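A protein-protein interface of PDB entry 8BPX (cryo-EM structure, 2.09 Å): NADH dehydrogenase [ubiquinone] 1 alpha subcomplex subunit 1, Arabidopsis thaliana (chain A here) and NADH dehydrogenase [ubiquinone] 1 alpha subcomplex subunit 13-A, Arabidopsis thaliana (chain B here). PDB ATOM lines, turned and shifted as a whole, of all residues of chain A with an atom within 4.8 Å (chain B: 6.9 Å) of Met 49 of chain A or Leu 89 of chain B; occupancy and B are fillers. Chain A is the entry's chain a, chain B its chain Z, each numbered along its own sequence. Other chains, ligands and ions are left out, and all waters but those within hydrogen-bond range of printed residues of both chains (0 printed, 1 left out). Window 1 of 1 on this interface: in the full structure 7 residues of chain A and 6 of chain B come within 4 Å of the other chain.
The guanidinium group of Arg 52 of chain A is in salt-bridge range of the side-chain carboxylate of Asp 53 of chain A (3.0 Å). NE1 of Trp 45 of chain A lies close to SD of Met 49 of chain A (3.7 Å).
The side-chain carboxylate (OE2) of Glu 92 of chain B is in salt-bridge range of the guanidinium group (NE) of Arg 52 of chain A, 2.6 Å away. The side-chain carboxylate of Asp 46 of chain A is in salt-bridge range of the guanidinium group of Arg 82 of chain B, 3.5 Å away.
Of the 9 printed residues of chain A, 4 touch a printed residue of chain B. Of the 11 printed residues of chain B, 4 touch a printed residue of chain A. Hydrophobic or aromatic side chains of chain B within 4 Å of the printed part of chain A: Ile 85 and Leu 89. Among the printed residues, 7 pairs touch across the chains.
Arg 82 of chain B touches Trp 45 of chain A. Trp 45 of chain A touches Ile 85 of chain B. Trp 45 of chain A touches Leu 89 of chain B. Met 49 of chain A touches Leu 89 of chain B (SD to CD1, 3.8 Å). Leu 89 of chain B touches Arg 52 of chain A (CD2 to NE, 3.5 Å).
Met 49 of chain A touches just one residue of chain B: Leu 89. Of chain A, only Trp 45 (3.7 Å), Met 49 (3.8 Å) and Arg 52 (3.5 Å) come within 4 Å of Leu 89 of chain B. Of the printed residues of chain A, Glu 92 of chain B touches Arg 52 (2.6 Å). Printed residues of chain A within 4 Å of Ile 85 of chain B: Trp 45. Of the printed residues of chain B, Asp 46 of chain A touches Arg 82. Ile 88 of chain B touches none of the printed residues of chain A.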
ATOM      1  N   TRP A  45      19.230  17.996   3.461  1.00  0.00           N
ATOM      2  CA  TRP A  45      19.046  17.652   2.056  1.00  0.00           C
ATOM      3  C   TRP A  45      20.317  17.063   1.458  1.00  0.00           C
ATOM      4  O   TRP A  45      20.268  16.054   0.746  1.00  0.00           O
ATOM      5  CB  TRP A  45      18.604  18.889   1.272  1.00  0.00           C
ATOM      6  CG  TRP A  45      18.400  18.632  -0.189  1.00  0.00           C
ATOM      7  CD1 TRP A  45      19.346  18.670  -1.167  1.00  0.00           C
ATOM      8  CD2 TRP A  45      17.166  18.297  -0.836  1.00  0.00           C
ATOM      9  NE1 TRP A  45      18.781  18.381  -2.386  1.00  0.00           N
ATOM     10  CE2 TRP A  45      17.443  18.149  -2.209  1.00  0.00           C
ATOM     11  CE3 TRP A  45      15.855  18.111  -0.387  1.00  0.00           C
ATOM     12  CZ2 TRP A  45      16.458  17.822  -3.138  1.00  0.00           C
ATOM     13  CZ3 TRP A  45      14.879  17.788  -1.311  1.00  0.00           C
ATOM     14  CH2 TRP A  45      15.186  17.644  -2.669  1.00  0.00           C
ATOM     15  N   ASP A  46      21.466  17.683   1.729  1.00  0.00           N
ATOM     16  CA  ASP A  46      22.721  17.194   1.162  1.00  0.00           C
ATOM     17  C   ASP A  46      23.074  15.812   1.703  1.00  0.00           C
ATOM     18  O   ASP A  46      23.549  14.949   0.956  1.00  0.00           O
ATOM     19  CB  ASP A  46      23.843  18.192   1.440  1.00  0.00           C
ATOM     20  CG  ASP A  46      23.606  19.535   0.777  1.00  0.00           C
ATOM     21  OD1 ASP A  46      23.214  19.559  -0.406  1.00  0.00           O
ATOM     22  OD2 ASP A  46      23.805  20.571   1.441  1.00  0.00           O
ATOM     23  N   VAL A  47      22.846  15.587   2.999  1.00  0.00           N
ATOM     24  CA  VAL A  47      23.118  14.283   3.598  1.00  0.00           C
ATOM     25  C   VAL A  47      22.223  13.211   2.985  1.00  0.00           C
ATOM     26  O   VAL A  47      22.682  12.107   2.657  1.00  0.00           O
ATOM     27  CB  VAL A  47      22.956  14.362   5.129  1.00  0.00           C
ATOM     28  CG1 VAL A  47      23.099  12.997   5.751  1.00  0.00           C
ATOM     29  CG2 VAL A  47      23.982  15.317   5.720  1.00  0.00           C
ATOM     30  N   ALA A  48      20.930  13.516   2.824  1.00  0.00           N
ATOM     31  CA  ALA A  48      20.023  12.569   2.181  1.00  0.00           C
ATOM     32  C   ALA A  48      20.433  12.305   0.735  1.00  0.00           C
ATOM     33  O   ALA A  48      20.346  11.169   0.255  1.00  0.00           O
ATOM     34  CB  ALA A  48      18.585  13.084   2.248  1.00  0.00           C
ATOM     35  N   MET A  49      20.889  13.343   0.030  1.00  0.00           N
ATOM     36  CA  MET A  49      21.369  13.175  -1.337  1.00  0.00           C
ATOM     37  C   MET A  49      22.562  12.233  -1.397  1.00  0.00           C
ATOM     38  O   MET A  49      22.618  11.346  -2.250  1.00  0.00           O
ATOM     39  CB  MET A  49      21.729  14.532  -1.944  1.00  0.00           C
ATOM     40  CG  MET A  49      20.580  15.454  -2.406  1.00  0.00           C
ATOM     41  SD  MET A  49      19.115  14.759  -3.224  1.00  0.00           S
ATOM     42  CE  MET A  49      18.191  14.004  -1.891  1.00  0.00           C
ATOM     43  N   GLU A  50      23.535  12.416  -0.502  1.00  0.00           N
ATOM     44  CA  GLU A  50      24.705  11.540  -0.496  1.00  0.00           C
ATOM     45  C   GLU A  50      24.331  10.100  -0.154  1.00  0.00           C
ATOM     46  O   GLU A  50      24.816   9.156  -0.797  1.00  0.00           O
ATOM     47  CB  GLU A  50      25.761  12.082   0.469  1.00  0.00           C
ATOM     48  CG  GLU A  50      26.376  13.404   0.027  1.00  0.00           C
ATOM     49  CD  GLU A  50      27.369  13.975   1.023  1.00  0.00           C
ATOM     50  OE1 GLU A  50      27.445  13.441   2.152  1.00  0.00           O
ATOM     51  OE2 GLU A  50      28.046  14.971   0.697  1.00  0.00           O
ATOM     52  N   ARG A  51      23.459   9.908   0.840  1.00  0.00           N
ATOM     53  CA  ARG A  51      23.060   8.551   1.200  1.00  0.00           C
ATOM     54  C   ARG A  51      22.316   7.867   0.057  1.00  0.00           C
ATOM     55  O   ARG A  51      22.553   6.687  -0.222  1.00  0.00           O
ATOM     56  CB  ARG A  51      22.208   8.558   2.470  1.00  0.00           C
ATOM     57  CG  ARG A  51      23.020   8.645   3.752  1.00  0.00           C
ATOM     58  CD  ARG A  51      22.266   9.394   4.834  1.00  0.00           C
ATOM     59  NE  ARG A  51      23.130   9.786   5.940  1.00  0.00           N
ATOM     60  CZ  ARG A  51      22.730   9.893   7.200  1.00  0.00           C
ATOM     61  NH1 ARG A  51      21.488   9.614   7.557  1.00  0.00           N
ATOM     62  NH2 ARG A  51      23.598  10.297   8.121  1.00  0.00           N
ATOM     63  N   ARG A  52      21.415   8.585  -0.619  1.00  0.00           N
ATOM     64  CA  ARG A  52      20.705   7.989  -1.747  1.00  0.00           C
ATOM     65  C   ARG A  52      21.628   7.780  -2.945  1.00  0.00           C
ATOM     66  O   ARG A  52      21.462   6.809  -3.698  1.00  0.00           O
ATOM     67  CB  ARG A  52      19.507   8.863  -2.114  1.00  0.00           C
ATOM     68  CG  ARG A  52      18.782   8.465  -3.376  1.00  0.00           C
ATOM     69  CD  ARG A  52      18.451   9.685  -4.205  1.00  0.00           C
ATOM     70  NE  ARG A  52      17.981   9.344  -5.541  1.00  0.00           N
ATOM     71  CZ  ARG A  52      18.629   9.641  -6.658  1.00  0.00           C
ATOM     72  NH1 ARG A  52      19.792  10.269  -6.636  1.00  0.00           N
ATOM     73  NH2 ARG A  52      18.098   9.296  -7.827  1.00  0.00           N
ATOM     74  N   ASP A  53      22.622   8.656  -3.118  1.00  0.00           N
ATOM     75  CA  ASP A  53      23.545   8.533  -4.238  1.00  0.00           C
ATOM     76  C   ASP A  53      24.462   7.336  -4.073  1.00  0.00           C
ATOM     77  O   ASP A  53      24.877   6.741  -5.072  1.00  0.00           O
ATOM     78  CB  ASP A  53      24.369   9.811  -4.389  1.00  0.00           C
ATOM     79  CG  ASP A  53      23.801  10.745  -5.436  1.00  0.00           C
ATOM     80  OD1 ASP A  53      22.595  10.632  -5.735  1.00  0.00           O
ATOM     81  OD2 ASP A  53      24.553  11.594  -5.955  1.00  0.00           O
ATOM     82  N   ARG B  82      15.929  22.553  -5.648  1.00  0.00           N
ATOM     83  CA  ARG B  82      15.489  21.418  -4.844  1.00  0.00           C
ATOM     84  C   ARG B  82      14.014  21.107  -5.063  1.00  0.00           C
ATOM     85  O   ARG B  82      13.599  19.948  -4.950  1.00  0.00           O
ATOM     86  CB  ARG B  82      15.765  21.678  -3.367  1.00  0.00           C
ATOM     87  CG  ARG B  82      17.223  21.533  -3.000  1.00  0.00           C
ATOM     88  CD  ARG B  82      17.508  22.101  -1.633  1.00  0.00           C
ATOM     89  NE  ARG B  82      18.915  21.968  -1.282  1.00  0.00           N
ATOM     90  CZ  ARG B  82      19.383  22.023  -0.045  1.00  0.00           C
ATOM     91  NH1 ARG B  82      18.583  22.236   0.987  1.00  0.00           N
ATOM     92  NH2 ARG B  82      20.685  21.853   0.163  1.00  0.00           N
ATOM     93  N   ILE B  85      13.237  18.881  -8.487  1.00  0.00           N
ATOM     94  CA  ILE B  85      13.633  17.475  -8.462  1.00  0.00           C
ATOM     95  C   ILE B  85      13.059  16.730  -7.269  1.00  0.00           C
ATOM     96  O   ILE B  85      13.325  15.531  -7.110  1.00  0.00           O
ATOM     97  CB  ILE B  85      15.167  17.322  -8.497  1.00  0.00           C
ATOM     98  CG1 ILE B  85      15.799  17.855  -7.207  1.00  0.00           C
ATOM     99  CG2 ILE B  85      15.743  18.010  -9.719  1.00  0.00           C
ATOM    100  CD1 ILE B  85      17.196  17.345  -6.962  1.00  0.00           C
ATOM    101  N   LEU B  86      12.278  17.404  -6.426  1.00  0.00           N
ATOM    102  CA  LEU B  86      11.627  16.733  -5.304  1.00  0.00           C
ATOM    103  C   LEU B  86      10.745  15.565  -5.737  1.00  0.00           C
ATOM    104  O   LEU B  86      10.862  14.480  -5.138  1.00  0.00           O
ATOM    105  CB  LEU B  86      10.835  17.773  -4.499  1.00  0.00           C
ATOM    106  CG  LEU B  86      10.073  17.396  -3.228  1.00  0.00           C
ATOM    107  CD1 LEU B  86       8.678  16.881  -3.520  1.00  0.00           C
ATOM    108  CD2 LEU B  86      10.838  16.381  -2.456  1.00  0.00           C
ATOM    109  N   PRO B  87       9.846  15.703  -6.723  1.00  0.00           N
ATOM    110  CA  PRO B  87       8.933  14.586  -7.026  1.00  0.00           C
ATOM    111  C   PRO B  87       9.620  13.289  -7.423  1.00  0.00           C
ATOM    112  O   PRO B  87       9.178  12.224  -6.984  1.00  0.00           O
ATOM    113  CB  PRO B  87       8.070  15.147  -8.164  1.00  0.00           C
ATOM    114  CG  PRO B  87       8.104  16.608  -7.960  1.00  0.00           C
ATOM    115  CD  PRO B  87       9.488  16.906  -7.499  1.00  0.00           C
ATOM    116  N   ILE B  88      10.689  13.335  -8.219  1.00  0.00           N
ATOM    117  CA  ILE B  88      11.320  12.088  -8.650  1.00  0.00           C
ATOM    118  C   ILE B  88      12.031  11.409  -7.483  1.00  0.00           C
ATOM    119  O   ILE B  88      11.982  10.180  -7.339  1.00  0.00           O
ATOM    120  CB  ILE B  88      12.265  12.331  -9.844  1.00  0.00           C
ATOM    121  CG1 ILE B  88      12.761  10.989 -10.389  1.00  0.00           C
ATOM    122  CG2 ILE B  88      13.426  13.250  -9.475  1.00  0.00           C
ATOM    123  CD1 ILE B  88      13.780  11.103 -11.479  1.00  0.00           C
ATOM    124  N   LEU B  89      12.683  12.192  -6.620  1.00  0.00           N
ATOM    125  CA  LEU B  89      13.301  11.616  -5.430  1.00  0.00           C
ATOM    126  C   LEU B  89      12.254  10.980  -4.525  1.00  0.00           C
ATOM    127  O   LEU B  89      12.453   9.871  -4.011  1.00  0.00           O
ATOM    128  CB  LEU B  89      14.087  12.693  -4.681  1.00  0.00           C
ATOM    129  CG  LEU B  89      15.203  13.367  -5.485  1.00  0.00           C
ATOM    130  CD1 LEU B  89      15.680  14.647  -4.808  1.00  0.00           C
ATOM    131  CD2 LEU B  89      16.366  12.406  -5.706  1.00  0.00           C
ATOM    132  N   GLN B  90      11.119  11.661  -4.338  1.00  0.00           N
ATOM    133  CA  GLN B  90      10.058  11.106  -3.506  1.00  0.00           C
ATOM    134  C   GLN B  90       9.479   9.834  -4.118  1.00  0.00           C
ATOM    135  O   GLN B  90       9.169   8.887  -3.396  1.00  0.00           O
ATOM    136  CB  GLN B  90       8.957  12.140  -3.286  1.00  0.00           C
ATOM    137  CG  GLN B  90       8.146  11.925  -2.019  1.00  0.00           C
ATOM    138  CD  GLN B  90       8.993  11.483  -0.842  1.00  0.00           C
ATOM    139  OE1 GLN B  90       9.785  12.258  -0.312  1.00  0.00           O
ATOM    140  NE2 GLN B  90       8.825  10.237  -0.422  1.00  0.00           N
ATOM    141  N   ALA B  91       9.313   9.804  -5.443  1.00  0.00           N
ATOM    142  CA  ALA B  91       8.775   8.614  -6.100  1.00  0.00           C
ATOM    143  C   ALA B  91       9.718   7.427  -5.949  1.00  0.00           C
ATOM    144  O   ALA B  91       9.278   6.301  -5.677  1.00  0.00           O
ATOM    145  CB  ALA B  91       8.514   8.909  -7.574  1.00  0.00           C
ATOM    146  N   GLU B  92      11.019   7.663  -6.125  1.00  0.00           N
ATOM    147  CA  GLU B  92      12.010   6.620  -5.880  1.00  0.00           C
ATOM    148  C   GLU B  92      11.920   6.107  -4.447  1.00  0.00           C
ATOM    149  O   GLU B  92      11.917   4.892  -4.205  1.00  0.00           O
ATOM    150  CB  GLU B  92      13.404   7.166  -6.166  1.00  0.00           C
ATOM    151  CG  GLU B  92      14.520   6.167  -6.002  1.00  0.00           C
ATOM    152  CD  GLU B  92      15.876   6.789  -6.258  1.00  0.00           C
ATOM    153  OE1 GLU B  92      16.268   6.895  -7.437  1.00  0.00           O
ATOM    154  OE2 GLU B  92      16.551   7.168  -5.280  1.00  0.00           O
ATOM    155  N   GLU B  93      11.842   7.027  -3.480  1.00  0.00           N
ATOM    156  CA  GLU B  93      11.753   6.616  -2.084  1.00  0.00           C
ATOM    157  C   GLU B  93      10.475   5.827  -1.820  1.00  0.00           C
ATOM    158  O   GLU B  93      10.481   4.864  -1.047  1.00  0.00           O
ATOM    159  CB  GLU B  93      11.836   7.836  -1.163  1.00  0.00           C
ATOM    160  CG  GLU B  93      11.486   7.548   0.293  1.00  0.00           C
ATOM    161  CD  GLU B  93      12.508   6.676   1.012  1.00  0.00           C
ATOM    162  OE1 GLU B  93      13.505   6.252   0.390  1.00  0.00           O
ATOM    163  OE2 GLU B  93      12.300   6.397   2.209  1.00  0.00           O
ATOM    164  N   ASP B  94       9.370   6.225  -2.452  1.00  0.00           N
ATOM    165  CA  ASP B  94       8.108   5.516  -2.265  1.00  0.00           C
ATOM    166  C   ASP B  94       8.199   4.090  -2.790  1.00  0.00           C
ATOM    167  O   ASP B  94       7.763   3.145  -2.126  1.00  0.00           O
ATOM    168  CB  ASP B  94       6.975   6.274  -2.957  1.00  0.00           C
ATOM    169  CG  ASP B  94       6.499   7.472  -2.161  1.00  0.00           C
ATOM    170  OD1 ASP B  94       6.992   7.673  -1.031  1.00  0.00           O
ATOM    171  OD2 ASP B  94       5.621   8.204  -2.661  1.00  0.00           O
